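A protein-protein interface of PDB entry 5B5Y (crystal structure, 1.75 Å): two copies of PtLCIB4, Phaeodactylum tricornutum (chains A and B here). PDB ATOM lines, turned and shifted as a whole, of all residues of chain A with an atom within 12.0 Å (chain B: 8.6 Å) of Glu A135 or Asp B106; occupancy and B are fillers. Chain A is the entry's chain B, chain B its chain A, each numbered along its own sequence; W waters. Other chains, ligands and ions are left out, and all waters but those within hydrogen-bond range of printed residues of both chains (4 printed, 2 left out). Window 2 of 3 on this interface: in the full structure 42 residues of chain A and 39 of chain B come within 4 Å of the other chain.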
ATOM      1  N   GLU A  64      -3.725  17.344 -22.629  1.00  0.00           N
ATOM      2  CA  GLU A  64      -4.489  16.150 -23.007  1.00  0.00           C
ATOM      3  C   GLU A  64      -5.976  16.244 -22.630  1.00  0.00           C
ATOM      4  O   GLU A  64      -6.795  15.551 -23.222  1.00  0.00           O
ATOM      5  CB  GLU A  64      -3.882  14.876 -22.389  1.00  0.00           C
ATOM      6  CG  GLU A  64      -4.089  14.699 -20.901  1.00  0.00           C
ATOM      7  CD  GLU A  64      -3.164  15.555 -20.040  1.00  0.00           C
ATOM      8  OE1 GLU A  64      -2.217  16.181 -20.574  1.00  0.00           O
ATOM      9  OE2 GLU A  64      -3.397  15.610 -18.811  1.00  0.00           O
ATOM     10  N   SER A 121     -13.031  22.515 -10.730  1.00  0.00           N
ATOM     11  CA  SER A 121     -12.895  21.355  -9.858  1.00  0.00           C
ATOM     12  C   SER A 121     -14.213  20.866  -9.264  1.00  0.00           C
ATOM     13  O   SER A 121     -15.280  21.457  -9.466  1.00  0.00           O
ATOM     14  CB  SER A 121     -11.929  21.676  -8.719  1.00  0.00           C
ATOM     15  OG  SER A 121     -12.528  22.554  -7.778  1.00  0.00           O
ATOM     16  N   TRP A 122     -14.119  19.783  -8.505  1.00  0.00           N
ATOM     17  CA  TRP A 122     -15.260  19.258  -7.766  1.00  0.00           C
ATOM     18  C   TRP A 122     -15.854  20.285  -6.803  1.00  0.00           C
ATOM     19  O   TRP A 122     -17.029  20.205  -6.458  1.00  0.00           O
ATOM     20  CB  TRP A 122     -14.851  18.006  -6.992  1.00  0.00           C
ATOM     21  CG  TRP A 122     -14.866  16.767  -7.811  1.00  0.00           C
ATOM     22  CD1 TRP A 122     -13.786  16.056  -8.259  1.00  0.00           C
ATOM     23  CD2 TRP A 122     -16.026  16.079  -8.290  1.00  0.00           C
ATOM     24  NE1 TRP A 122     -14.207  14.965  -8.985  1.00  0.00           N
ATOM     25  CE2 TRP A 122     -15.578  14.958  -9.019  1.00  0.00           C
ATOM     26  CE3 TRP A 122     -17.403  16.304  -8.173  1.00  0.00           C
ATOM     27  CZ2 TRP A 122     -16.457  14.064  -9.625  1.00  0.00           C
ATOM     28  CZ3 TRP A 122     -18.272  15.416  -8.777  1.00  0.00           C
ATOM     29  CH2 TRP A 122     -17.796  14.312  -9.495  1.00  0.00           C
ATOM     30  N   GLU A 123     -15.033  21.235  -6.366  1.00  0.00           N
ATOM     31  CA  GLU A 123     -15.474  22.284  -5.451  1.00  0.00           C
ATOM     32  C   GLU A 123     -15.972  23.528  -6.190  1.00  0.00           C
ATOM     33  O   GLU A 123     -16.307  24.537  -5.566  1.00  0.00           O
ATOM     34  CB  GLU A 123     -14.332  22.675  -4.510  1.00  0.00           C
ATOM     35  CG  GLU A 123     -13.758  21.520  -3.708  1.00  0.00           C
ATOM     36  CD  GLU A 123     -12.289  21.722  -3.380  1.00  0.00           C
ATOM     37  OE1 GLU A 123     -11.723  22.760  -3.785  1.00  0.00           O
ATOM     38  OE2 GLU A 123     -11.699  20.843  -2.718  1.00  0.00           O
ATOM     39  N   LYS A 125     -14.119  25.332  -8.184  1.00  0.00           N
ATOM     40  CA  LYS A 125     -13.010  26.279  -8.202  1.00  0.00           C
ATOM     41  C   LYS A 125     -12.389  26.328  -9.596  1.00  0.00           C
ATOM     42  O   LYS A 125     -12.047  25.284 -10.150  1.00  0.00           O
ATOM     43  CB  LYS A 125     -11.964  25.873  -7.162  1.00  0.00           C
ATOM     44  CG  LYS A 125     -10.698  26.697  -7.150  1.00  0.00           C
ATOM     45  CD  LYS A 125      -9.631  25.993  -6.326  1.00  0.00           C
ATOM     46  CE  LYS A 125      -8.276  26.653  -6.461  1.00  0.00           C
ATOM     47  NZ  LYS A 125      -7.193  25.704  -6.077  1.00  0.00           N
ATOM     48  N   THR A 128      -8.363  24.906 -12.283  1.00  0.00           N
ATOM     49  CA  THR A 128      -7.824  23.603 -11.913  1.00  0.00           C
ATOM     50  C   THR A 128      -8.884  22.520 -12.073  1.00  0.00           C
ATOM     51  O   THR A 128     -10.088  22.786 -11.977  1.00  0.00           O
ATOM     52  CB  THR A 128      -7.274  23.594 -10.459  1.00  0.00           C
ATOM     53  OG1 THR A 128      -6.656  22.327 -10.177  1.00  0.00           O
ATOM     54  CG2 THR A 128      -8.401  23.840  -9.446  1.00  0.00           C
ATOM     55  N   VAL A 129      -8.430  21.303 -12.337  1.00  0.00           N
ATOM     56  CA  VAL A 129      -9.313  20.148 -12.422  1.00  0.00           C
ATOM     57  C   VAL A 129      -8.523  18.888 -12.076  1.00  0.00           C
ATOM     58  O   VAL A 129      -7.323  18.795 -12.357  1.00  0.00           O
ATOM     59  CB  VAL A 129      -9.981  20.019 -13.832  1.00  0.00           C
ATOM     60  CG1 VAL A 129      -8.956  19.704 -14.907  1.00  0.00           C
ATOM     61  CG2 VAL A 129     -11.087  18.962 -13.826  1.00  0.00           C
ATOM     62  N   ALA A 130      -9.187  17.930 -11.435  1.00  0.00           N
ATOM     63  CA  ALA A 130      -8.563  16.649 -11.149  1.00  0.00           C
ATOM     64  C   ALA A 130      -8.094  15.986 -12.440  1.00  0.00           C
ATOM     65  O   ALA A 130      -8.786  16.028 -13.460  1.00  0.00           O
ATOM     66  CB  ALA A 130      -9.526  15.734 -10.405  1.00  0.00           C
ATOM     67  N   ARG A 131      -6.904  15.401 -12.392  1.00  0.00           N
ATOM     68  CA  ARG A 131      -6.370  14.661 -13.524  1.00  0.00           C
ATOM     69  C   ARG A 131      -6.197  13.187 -13.195  1.00  0.00           C
ATOM     70  O   ARG A 131      -5.797  12.837 -12.085  1.00  0.00           O
ATOM     71  CB  ARG A 131      -5.034  15.257 -13.963  1.00  0.00           C
ATOM     72  CG  ARG A 131      -5.166  16.666 -14.505  1.00  0.00           C
ATOM     73  CD  ARG A 131      -3.827  17.255 -14.883  1.00  0.00           C
ATOM     74  NE  ARG A 131      -3.982  18.651 -15.281  1.00  0.00           N
ATOM     75  CZ  ARG A 131      -4.184  19.050 -16.531  1.00  0.00           C
ATOM     76  NH1 ARG A 131      -4.221  18.155 -17.511  1.00  0.00           N
ATOM     77  NH2 ARG A 131      -4.322  20.345 -16.797  1.00  0.00           N
ATOM     78  N   ARG A 132      -6.496  12.333 -14.168  1.00  0.00           N
ATOM     79  CA  ARG A 132      -6.331  10.883 -14.026  1.00  0.00           C
ATOM     80  C   ARG A 132      -5.007  10.483 -13.358  1.00  0.00           C
ATOM     81  O   ARG A 132      -3.928  10.923 -13.756  1.00  0.00           O
ATOM     82  CB  ARG A 132      -6.456  10.212 -15.403  1.00  0.00           C
ATOM     83  CG  ARG A 132      -6.013   8.754 -15.440  1.00  0.00           C
ATOM     84  CD  ARG A 132      -6.148   8.140 -16.840  1.00  0.00           C
ATOM     85  NE  ARG A 132      -5.293   8.770 -17.853  1.00  0.00           N
ATOM     86  CZ  ARG A 132      -4.033   8.415 -18.108  1.00  0.00           C
ATOM     87  NH1 ARG A 132      -3.453   7.434 -17.419  1.00  0.00           N
ATOM     88  NH2 ARG A 132      -3.343   9.041 -19.059  1.00  0.00           N
ATOM     89  N   GLY A 133      -5.100   9.675 -12.309  1.00  0.00           N
ATOM     90  CA  GLY A 133      -3.917   9.147 -11.653  1.00  0.00           C
ATOM     91  C   GLY A 133      -3.116  10.096 -10.780  1.00  0.00           C
ATOM     92  O   GLY A 133      -2.051   9.722 -10.291  1.00  0.00           O
ATOM     93  N   ARG A 134      -3.614  11.315 -10.574  1.00  0.00           N
ATOM     94  CA  ARG A 134      -2.914  12.297  -9.746  1.00  0.00           C
ATOM     95  C   ARG A 134      -3.745  12.744  -8.554  1.00  0.00           C
ATOM     96  O   ARG A 134      -4.956  12.893  -8.669  1.00  0.00           O
ATOM     97  CB  ARG A 134      -2.537  13.539 -10.559  1.00  0.00           C
ATOM     98  CG  ARG A 134      -1.575  13.294 -11.678  1.00  0.00           C
ATOM     99  CD  ARG A 134      -1.139  14.615 -12.268  1.00  0.00           C
ATOM    100  NE  ARG A 134       0.304  14.635 -12.406  1.00  0.00           N
ATOM    101  CZ  ARG A 134       1.131  15.157 -11.511  1.00  0.00           C
ATOM    102  NH1 ARG A 134       0.659  15.736 -10.423  1.00  0.00           N
ATOM    103  NH2 ARG A 134       2.430  15.111 -11.724  1.00  0.00           N
ATOM    104  N   GLU A 135      -3.080  12.994  -7.429  1.00  0.00           N
ATOM    105  CA  GLU A 135      -3.749  13.546  -6.256  1.00  0.00           C
ATOM    106  C   GLU A 135      -3.914  15.054  -6.426  1.00  0.00           C
ATOM    107  O   GLU A 135      -4.926  15.624  -6.020  1.00  0.00           O
ATOM    108  CB  GLU A 135      -2.964  13.229  -4.979  1.00  0.00           C
ATOM    109  CG  GLU A 135      -3.841  12.907  -3.764  1.00  0.00           C
ATOM    110  CD  GLU A 135      -3.908  14.042  -2.744  1.00  0.00           C
ATOM    111  OE1 GLU A 135      -3.255  15.088  -2.954  1.00  0.00           O
ATOM    112  OE2 GLU A 135      -4.632  13.890  -1.732  1.00  0.00           O
ATOM    113  N   LYS A 136      -2.906  15.685  -7.025  1.00  0.00           N
ATOM    114  CA  LYS A 136      -2.942  17.115  -7.318  1.00  0.00           C
ATOM    115  C   LYS A 136      -2.952  17.356  -8.832  1.00  0.00           C
ATOM    116  O   LYS A 136      -2.038  16.937  -9.547  1.00  0.00           O
ATOM    117  CB  LYS A 136      -1.746  17.827  -6.679  1.00  0.00           C
ATOM    118  CG  LYS A 136      -1.649  17.673  -5.166  1.00  0.00           C
ATOM    119  CD  LYS A 136      -0.440  18.417  -4.617  1.00  0.00           C
ATOM    120  CE  LYS A 136      -0.276  18.198  -3.117  1.00  0.00           C
ATOM    121  NZ  LYS A 136       1.019  18.760  -2.621  1.00  0.00           N
ATOM    122  N   GLY A 137      -3.984  18.038  -9.314  1.00  0.00           N
ATOM    123  CA  GLY A 137      -4.148  18.247 -10.742  1.00  0.00           C
ATOM    124  C   GLY A 137      -3.319  19.372 -11.333  1.00  0.00           C
ATOM    125  O   GLY A 137      -3.055  19.394 -12.536  1.00  0.00           O
ATOM    126  N   GLY A 138      -2.905  20.312 -10.494  1.00  0.00           N
ATOM    127  CA  GLY A 138      -2.182  21.470 -10.980  1.00  0.00           C
ATOM    128  C   GLY A 138      -3.089  22.393 -11.772  1.00  0.00           C
ATOM    129  O   GLY A 138      -4.322  22.272 -11.718  1.00  0.00           O
ATOM    130  N   ALA A 139      -2.480  23.306 -12.518  1.00  0.00           N
ATOM    131  CA  ALA A 139      -3.233  24.353 -13.194  1.00  0.00           C
ATOM    132  C   ALA A 139      -3.819  23.883 -14.515  1.00  0.00           C
ATOM    133  O   ALA A 139      -3.268  23.019 -15.196  1.00  0.00           O
ATOM    134  CB  ALA A 139      -2.354  25.580 -13.415  1.00  0.00           C
ATOM    135  N   PRO A 251     -14.239  17.466 -14.038  1.00  0.00           N
ATOM    136  CA  PRO A 251     -13.748  16.124 -13.687  1.00  0.00           C
ATOM    137  C   PRO A 251     -14.254  15.051 -14.656  1.00  0.00           C
ATOM    138  O   PRO A 251     -15.339  15.208 -15.221  1.00  0.00           O
ATOM    139  CB  PRO A 251     -14.309  15.913 -12.278  1.00  0.00           C
ATOM    140  CG  PRO A 251     -14.367  17.295 -11.715  1.00  0.00           C
ATOM    141  CD  PRO A 251     -14.769  18.182 -12.864  1.00  0.00           C
ATOM    142  N   LYS A 252     -13.477  13.987 -14.839  1.00  0.00           N
ATOM    143  CA  LYS A 252     -13.751  12.990 -15.878  1.00  0.00           C
ATOM    144  C   LYS A 252     -15.137  12.328 -15.783  1.00  0.00           C
ATOM    145  O   LYS A 252     -15.687  11.885 -16.790  1.00  0.00           O
ATOM    146  CB  LYS A 252     -12.663  11.906 -15.866  1.00  0.00           C
ATOM    147  CG  LYS A 252     -12.566  11.101 -14.578  1.00  0.00           C
ATOM    148  CD  LYS A 252     -11.601   9.931 -14.733  1.00  0.00           C
ATOM    149  CE  LYS A 252     -11.438   9.161 -13.428  1.00  0.00           C
ATOM    150  NZ  LYS A 252     -10.680   9.931 -12.398  1.00  0.00           N
ATOM    151  N   GLU A 253     -15.704  12.273 -14.584  1.00  0.00           N
ATOM    152  CA  GLU A 253     -17.020  11.661 -14.381  1.00  0.00           C
ATOM    153  C   GLU A 253     -18.145  12.574 -14.850  1.00  0.00           C
ATOM    154  O   GLU A 253     -19.321  12.222 -14.769  1.00  0.00           O
ATOM    155  CB  GLU A 253     -17.240  11.306 -12.906  1.00  0.00           C
ATOM    156  CG  GLU A 253     -16.067  10.609 -12.224  1.00  0.00           C
ATOM    157  CD  GLU A 253     -14.925  11.554 -11.875  1.00  0.00           C
ATOM    158  OE1 GLU A 253     -15.124  12.784 -11.946  1.00  0.00           O
ATOM    159  OE2 GLU A 253     -13.831  11.063 -11.527  1.00  0.00           O
ATOM    160  N   TYR B  52      -3.059   2.699 -17.029  1.00  0.00           N
ATOM    161  CA  TYR B  52      -3.431   3.609 -15.943  1.00  0.00           C
ATOM    162  C   TYR B  52      -2.305   4.546 -15.529  1.00  0.00           C
ATOM    163  O   TYR B  52      -2.572   5.629 -15.016  1.00  0.00           O
ATOM    164  CB  TYR B  52      -3.905   2.831 -14.706  1.00  0.00           C
ATOM    165  CG  TYR B  52      -2.792   2.352 -13.794  1.00  0.00           C
ATOM    166  CD1 TYR B  52      -2.108   1.171 -14.062  1.00  0.00           C
ATOM    167  CD2 TYR B  52      -2.437   3.068 -12.654  1.00  0.00           C
ATOM    168  CE1 TYR B  52      -1.088   0.726 -13.230  1.00  0.00           C
ATOM    169  CE2 TYR B  52      -1.415   2.632 -11.815  1.00  0.00           C
ATOM    170  CZ  TYR B  52      -0.747   1.456 -12.107  1.00  0.00           C
ATOM    171  OH  TYR B  52       0.269   1.007 -11.283  1.00  0.00           O
ATOM    172  N   ASN B  53      -1.055   4.136 -15.746  1.00  0.00           N
ATOM    173  CA  ASN B  53       0.076   4.877 -15.199  1.00  0.00           C
ATOM    174  C   ASN B  53       0.979   5.488 -16.257  1.00  0.00           C
ATOM    175  O   ASN B  53       2.084   5.914 -15.943  1.00  0.00           O
ATOM    176  CB  ASN B  53       0.925   3.987 -14.290  1.00  0.00           C
ATOM    177  CG  ASN B  53       1.609   2.849 -15.046  1.00  0.00           C
ATOM    178  OD1 ASN B  53       1.166   2.439 -16.122  1.00  0.00           O
ATOM    179  ND2 ASN B  53       2.685   2.328 -14.472  1.00  0.00           N
ATOM    180  N   THR B  54       0.513   5.499 -17.496  1.00  0.00           N
ATOM    181  CA  THR B  54       1.288   6.076 -18.602  1.00  0.00           C
ATOM    182  C   THR B  54       0.545   7.253 -19.219  1.00  0.00           C
ATOM    183  O   THR B  54      -0.626   7.129 -19.548  1.00  0.00           O
ATOM    184  CB  THR B  54       1.561   5.026 -19.688  1.00  0.00           C
ATOM    185  OG1 THR B  54       2.290   3.929 -19.120  1.00  0.00           O
ATOM    186  CG2 THR B  54       2.374   5.634 -20.866  1.00  0.00           C
ATOM    187  N   ALA B 101       4.762  16.824 -18.134  1.00  0.00           N
ATOM    188  CA  ALA B 101       5.337  16.130 -16.975  1.00  0.00           C
ATOM    189  C   ALA B 101       4.471  16.295 -15.728  1.00  0.00           C
ATOM    190  O   ALA B 101       4.314  15.359 -14.942  1.00  0.00           O
ATOM    191  CB  ALA B 101       6.748  16.630 -16.701  1.00  0.00           C
ATOM    192  N   GLY B 102       3.903  17.443 -15.544  1.00  0.00           N
ATOM    193  CA  GLY B 102       3.034  17.694 -14.421  1.00  0.00           C
ATOM    194  C   GLY B 102       1.677  17.030 -14.507  1.00  0.00           C
ATOM    195  O   GLY B 102       0.885  17.192 -13.620  1.00  0.00           O
ATOM    196  N   HIS B 103       1.427  16.325 -15.597  1.00  0.00           N
ATOM    197  CA  HIS B 103       0.188  15.615 -15.832  1.00  0.00           C
ATOM    198  C   HIS B 103       0.389  14.100 -15.737  1.00  0.00           C
ATOM    199  O   HIS B 103      -0.540  13.396 -15.825  1.00  0.00           O
ATOM    200  CB  HIS B 103      -0.424  15.871 -17.219  1.00  0.00           C
ATOM    201  CG  HIS B 103      -0.768  17.288 -17.513  1.00  0.00           C
ATOM    202  ND1 HIS B 103      -0.756  18.283 -16.571  1.00  0.00           N
ATOM    203  CD2 HIS B 103      -1.121  17.875 -18.669  1.00  0.00           C
ATOM    204  CE1 HIS B 103      -1.073  19.422 -17.139  1.00  0.00           C
ATOM    205  NE2 HIS B 103      -1.278  19.202 -18.416  1.00  0.00           N
ATOM    206  N   ILE B 104       1.619  13.643 -15.592  1.00  0.00           N
ATOM    207  CA  ILE B 104       1.897  12.218 -15.502  1.00  0.00           C
ATOM    208  C   ILE B 104       1.284  11.634 -14.221  1.00  0.00           C
ATOM    209  O   ILE B 104       1.417  12.221 -13.152  1.00  0.00           O
ATOM    210  CB  ILE B 104       3.411  11.952 -15.527  1.00  0.00           C
ATOM    211  CG1 ILE B 104       3.998  12.378 -16.879  1.00  0.00           C
ATOM    212  CG2 ILE B 104       3.718  10.470 -15.228  1.00  0.00           C
ATOM    213  CD1 ILE B 104       5.513  12.345 -16.913  1.00  0.00           C
ATOM    214  N   PRO B 105       0.571  10.503 -14.339  1.00  0.00           N
ATOM    215  CA  PRO B 105       0.016   9.834 -13.153  1.00  0.00           C
ATOM    216  C   PRO B 105       1.073   9.660 -12.064  1.00  0.00           C
ATOM    217  O   PRO B 105       2.228   9.398 -12.387  1.00  0.00           O
ATOM    218  CB  PRO B 105      -0.435   8.481 -13.699  1.00  0.00           C
ATOM    219  CG  PRO B 105      -0.789   8.758 -15.116  1.00  0.00           C
ATOM    220  CD  PRO B 105       0.189   9.818 -15.585  1.00  0.00           C
ATOM    221  N   ASP B 106       0.686   9.833 -10.802  1.00  0.00           N
ATOM    222  CA  ASP B 106       1.629   9.686  -9.694  1.00  0.00           C
ATOM    223  C   ASP B 106       2.348   8.341  -9.781  1.00  0.00           C
ATOM    224  O   ASP B 106       1.722   7.307  -9.984  1.00  0.00           O
ATOM    225  CB  ASP B 106       0.916   9.814  -8.341  1.00  0.00           C
ATOM    226  CG  ASP B 106       0.285  11.184  -8.130  1.00  0.00           C
ATOM    227  OD1 ASP B 106       0.797  12.182  -8.686  1.00  0.00           O
ATOM    228  OD2 ASP B 106      -0.716  11.263  -7.382  1.00  0.00           O
ATOM    229  N   GLY B 107       3.670   8.372  -9.664  1.00  0.00           N
ATOM    230  CA  GLY B 107       4.463   7.158  -9.742  1.00  0.00           C
ATOM    231  C   GLY B 107       4.541   6.555 -11.137  1.00  0.00           C
ATOM    232  O   GLY B 107       5.048   5.447 -11.308  1.00  0.00           O
ATOM    233  N   GLY B 108       4.052   7.287 -12.134  1.00  0.00           N
ATOM    234  CA  GLY B 108       4.019   6.787 -13.498  1.00  0.00           C
ATOM    235  C   GLY B 108       5.057   7.407 -14.416  1.00  0.00           C
ATOM    236  O   GLY B 108       5.997   8.071 -13.966  1.00  0.00           O
ATOM    237  N   SER B 109       4.871   7.199 -15.717  1.00  0.00           N
ATOM    238  CA  SER B 109       5.850   7.621 -16.709  1.00  0.00           C
ATOM    239  C   SER B 109       5.169   8.194 -17.937  1.00  0.00           C
ATOM    240  O   SER B 109       3.956   8.094 -18.086  1.00  0.00           O
ATOM    241  CB  SER B 109       6.740   6.440 -17.114  1.00  0.00           C
ATOM    242  OG  SER B 109       7.564   6.026 -16.036  1.00  0.00           O
ATOM    243  N   ASP B 235      10.360  13.213 -11.735  1.00  0.00           N
ATOM    244  CA  ASP B 235      10.871  12.895 -10.404  1.00  0.00           C
ATOM    245  C   ASP B 235      10.893  11.397 -10.090  1.00  0.00           C
ATOM    246  O   ASP B 235      10.194  10.602 -10.718  1.00  0.00           O
ATOM    247  CB  ASP B 235      10.051  13.626  -9.337  1.00  0.00           C
ATOM    248  CG  ASP B 235      10.783  14.828  -8.765  1.00  0.00           C
ATOM    249  OD1 ASP B 235      11.993  14.979  -9.045  1.00  0.00           O
ATOM    250  OD2 ASP B 235      10.152  15.620  -8.032  1.00  0.00           O
ATOM    251  N   ASP B 237      11.004   7.601  -9.452  1.00  0.00           N
ATOM    252  CA  ASP B 237      11.083   6.426 -10.310  1.00  0.00           C
ATOM    253  C   ASP B 237      10.462   6.693 -11.677  1.00  0.00           C
ATOM    254  O   ASP B 237      10.417   5.803 -12.522  1.00  0.00           O
ATOM    255  CB  ASP B 237      10.389   5.229  -9.655  1.00  0.00           C
ATOM    256  CG  ASP B 237      10.934   4.921  -8.272  1.00  0.00           C
ATOM    257  OD1 ASP B 237      12.169   5.004  -8.078  1.00  0.00           O
ATOM    258  OD2 ASP B 237      10.122   4.598  -7.377  1.00  0.00           O
ATOM    259  N   GLY B 238       9.979   7.915 -11.883  1.00  0.00           N
ATOM    260  CA  GLY B 238       9.329   8.270 -13.136  1.00  0.00           C
ATOM    261  C   GLY B 238      10.293   8.151 -14.299  1.00  0.00           C
ATOM    262  O   GLY B 238      11.491   8.394 -14.146  1.00  0.00           O
HETATM  263  O   HOH W   1      -1.132  22.404 -17.525  1.00  0.00           O
HETATM  264  O   HOH W   2       4.917  14.574 -12.228  1.00  0.00           O
HETATM  265  O   HOH W   3      -3.120  12.518 -15.905  1.00  0.00           O
HETATM  266  O   HOH W   4      -1.281  20.943 -14.512  1.00  0.00           O
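The backbone carbonyl oxygen (O) of Tyr B52 sits at hydrogen-bond distance from the guanidinium group (NH1) of Arg A132 (3.1 Å).
The backbone carbonyl oxygen (O) of Thr B54 lies within hydrogen-bond range of the guanidinium group (NH2) of Arg A132 (3.4 Å).
The guanidinium group (NE) of Arg A134 is in hydrogen-bond range of the backbone carbonyl oxygen (O) of Gly B102, at 2.9 Å.
A ring nitrogen (NE2) of His B103 sits at hydrogen-bond distance from the guanidinium group of Arg A131.
O of Ile B104 is in hydrogen-bond range of NE of Arg A134 (2.8 Å).
O of Gly A133 sits at hydrogen-bond distance from N of Asp B106.
The side-chain carboxylate of Asp B106 is in salt-bridge range of the guanidinium group of Arg A134, at 3.96 Å.
OD2 of Asp B106 lies within hydrogen-bond range of N of Glu A135 (2.9 Å).
The guanidinium group of Arg A131 lies within salt-bridge range of the side-chain carboxylate of Glu A64, 3.0 Å away.
NE of Arg A131 lies within hydrogen-bond range of O of Gly A137 (3.0 Å).
NH2 of Arg A131 is in hydrogen-bond range of O of Ala A139, 3.3 Å away.
NH1 of Arg A134 is in hydrogen-bond range of O of Lys A136.
His B103 touches Glu A64 (CD2 to OE1, 2.8 Å).
Pro B105 touches Arg A132 (CG to NH1, 3.8 Å).
O of Gly A133 touches CA of Pro B105 (3.5 Å).
Ala B101 touches Arg A134 (O to NH2, 3.7 Å).
His B103 touches Arg A134 (C to NE, 3.4 Å).
Of the printed residues of chain B, Glu A135 touches Asp B106 (2.9 Å).
Asp B106 touches three residues of chain A.
No residue of chain A comes within 4 Å of Asn B53.
No residue of chain A comes within 4 Å of Gly B107.
No residue of chain A comes within 4 Å of Gly B108.
Of the printed residues of chain A, Thr B54 touches Arg A132.
Printed residues of chain A within 4 Å of Ile B104: Arg A134.
Of the printed residues of chain A, His B103 touches Glu A64 (2.8 Å), Arg A131 (3.2 Å) and Arg A134 (3.4 Å).
Of the printed residues of chain B, Gly A133 touches Pro B105 and Asp B106.
Printed residues of chain B within 4 Å of Glu A64: His B103 (2.8 Å).
Glu A253 touches none of the printed residues of chain B.
Ala A139 touches none of the printed residues of chain B.
The nearest residue of chain B that does not touch Glu A135 is Pro B105 (7.1 Å).
The nearest residue of chain A that does not touch Asp B106 is Lys A136 (4.9 Å).
Of the 15 printed residues of chain B, 8 touch a printed residue of chain A.
Printed residues of chain B that touch a printed residue of chain A: Tyr B52, Thr B54, Ala B101, Gly B102, His B103, Ile B104, Pro B105 and Asp B106.
Of the 20 printed residues of chain A, 6 touch a printed residue of chain B.
Among the printed residues, 13 pairs touch across the chains.
No position is printed for both chains.
Of the 13 pairs that touch across the chains among the printed residues, none has its exchanged pair printed and touching as well.
Water W2 bridges the guanidinium group of Arg A134 (2.6 Å) and the backbone carbonyl oxygen of Ala B101 (2.9 Å).
Water W3 bridges O of His B103 (2.7 Å) and O of Arg A132 (2.8 Å).
Water W4 lies within hydrogen-bond range of O of Ala A139 (3.0 Å), O of Gly A137 (3.1 Å) and ND1 of His B103 (3.4 Å).
Water W1 lies within hydrogen-bond range of the backbone carbonyl oxygen of Ala A139 and a ring nitrogen (NE2) of His B103.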
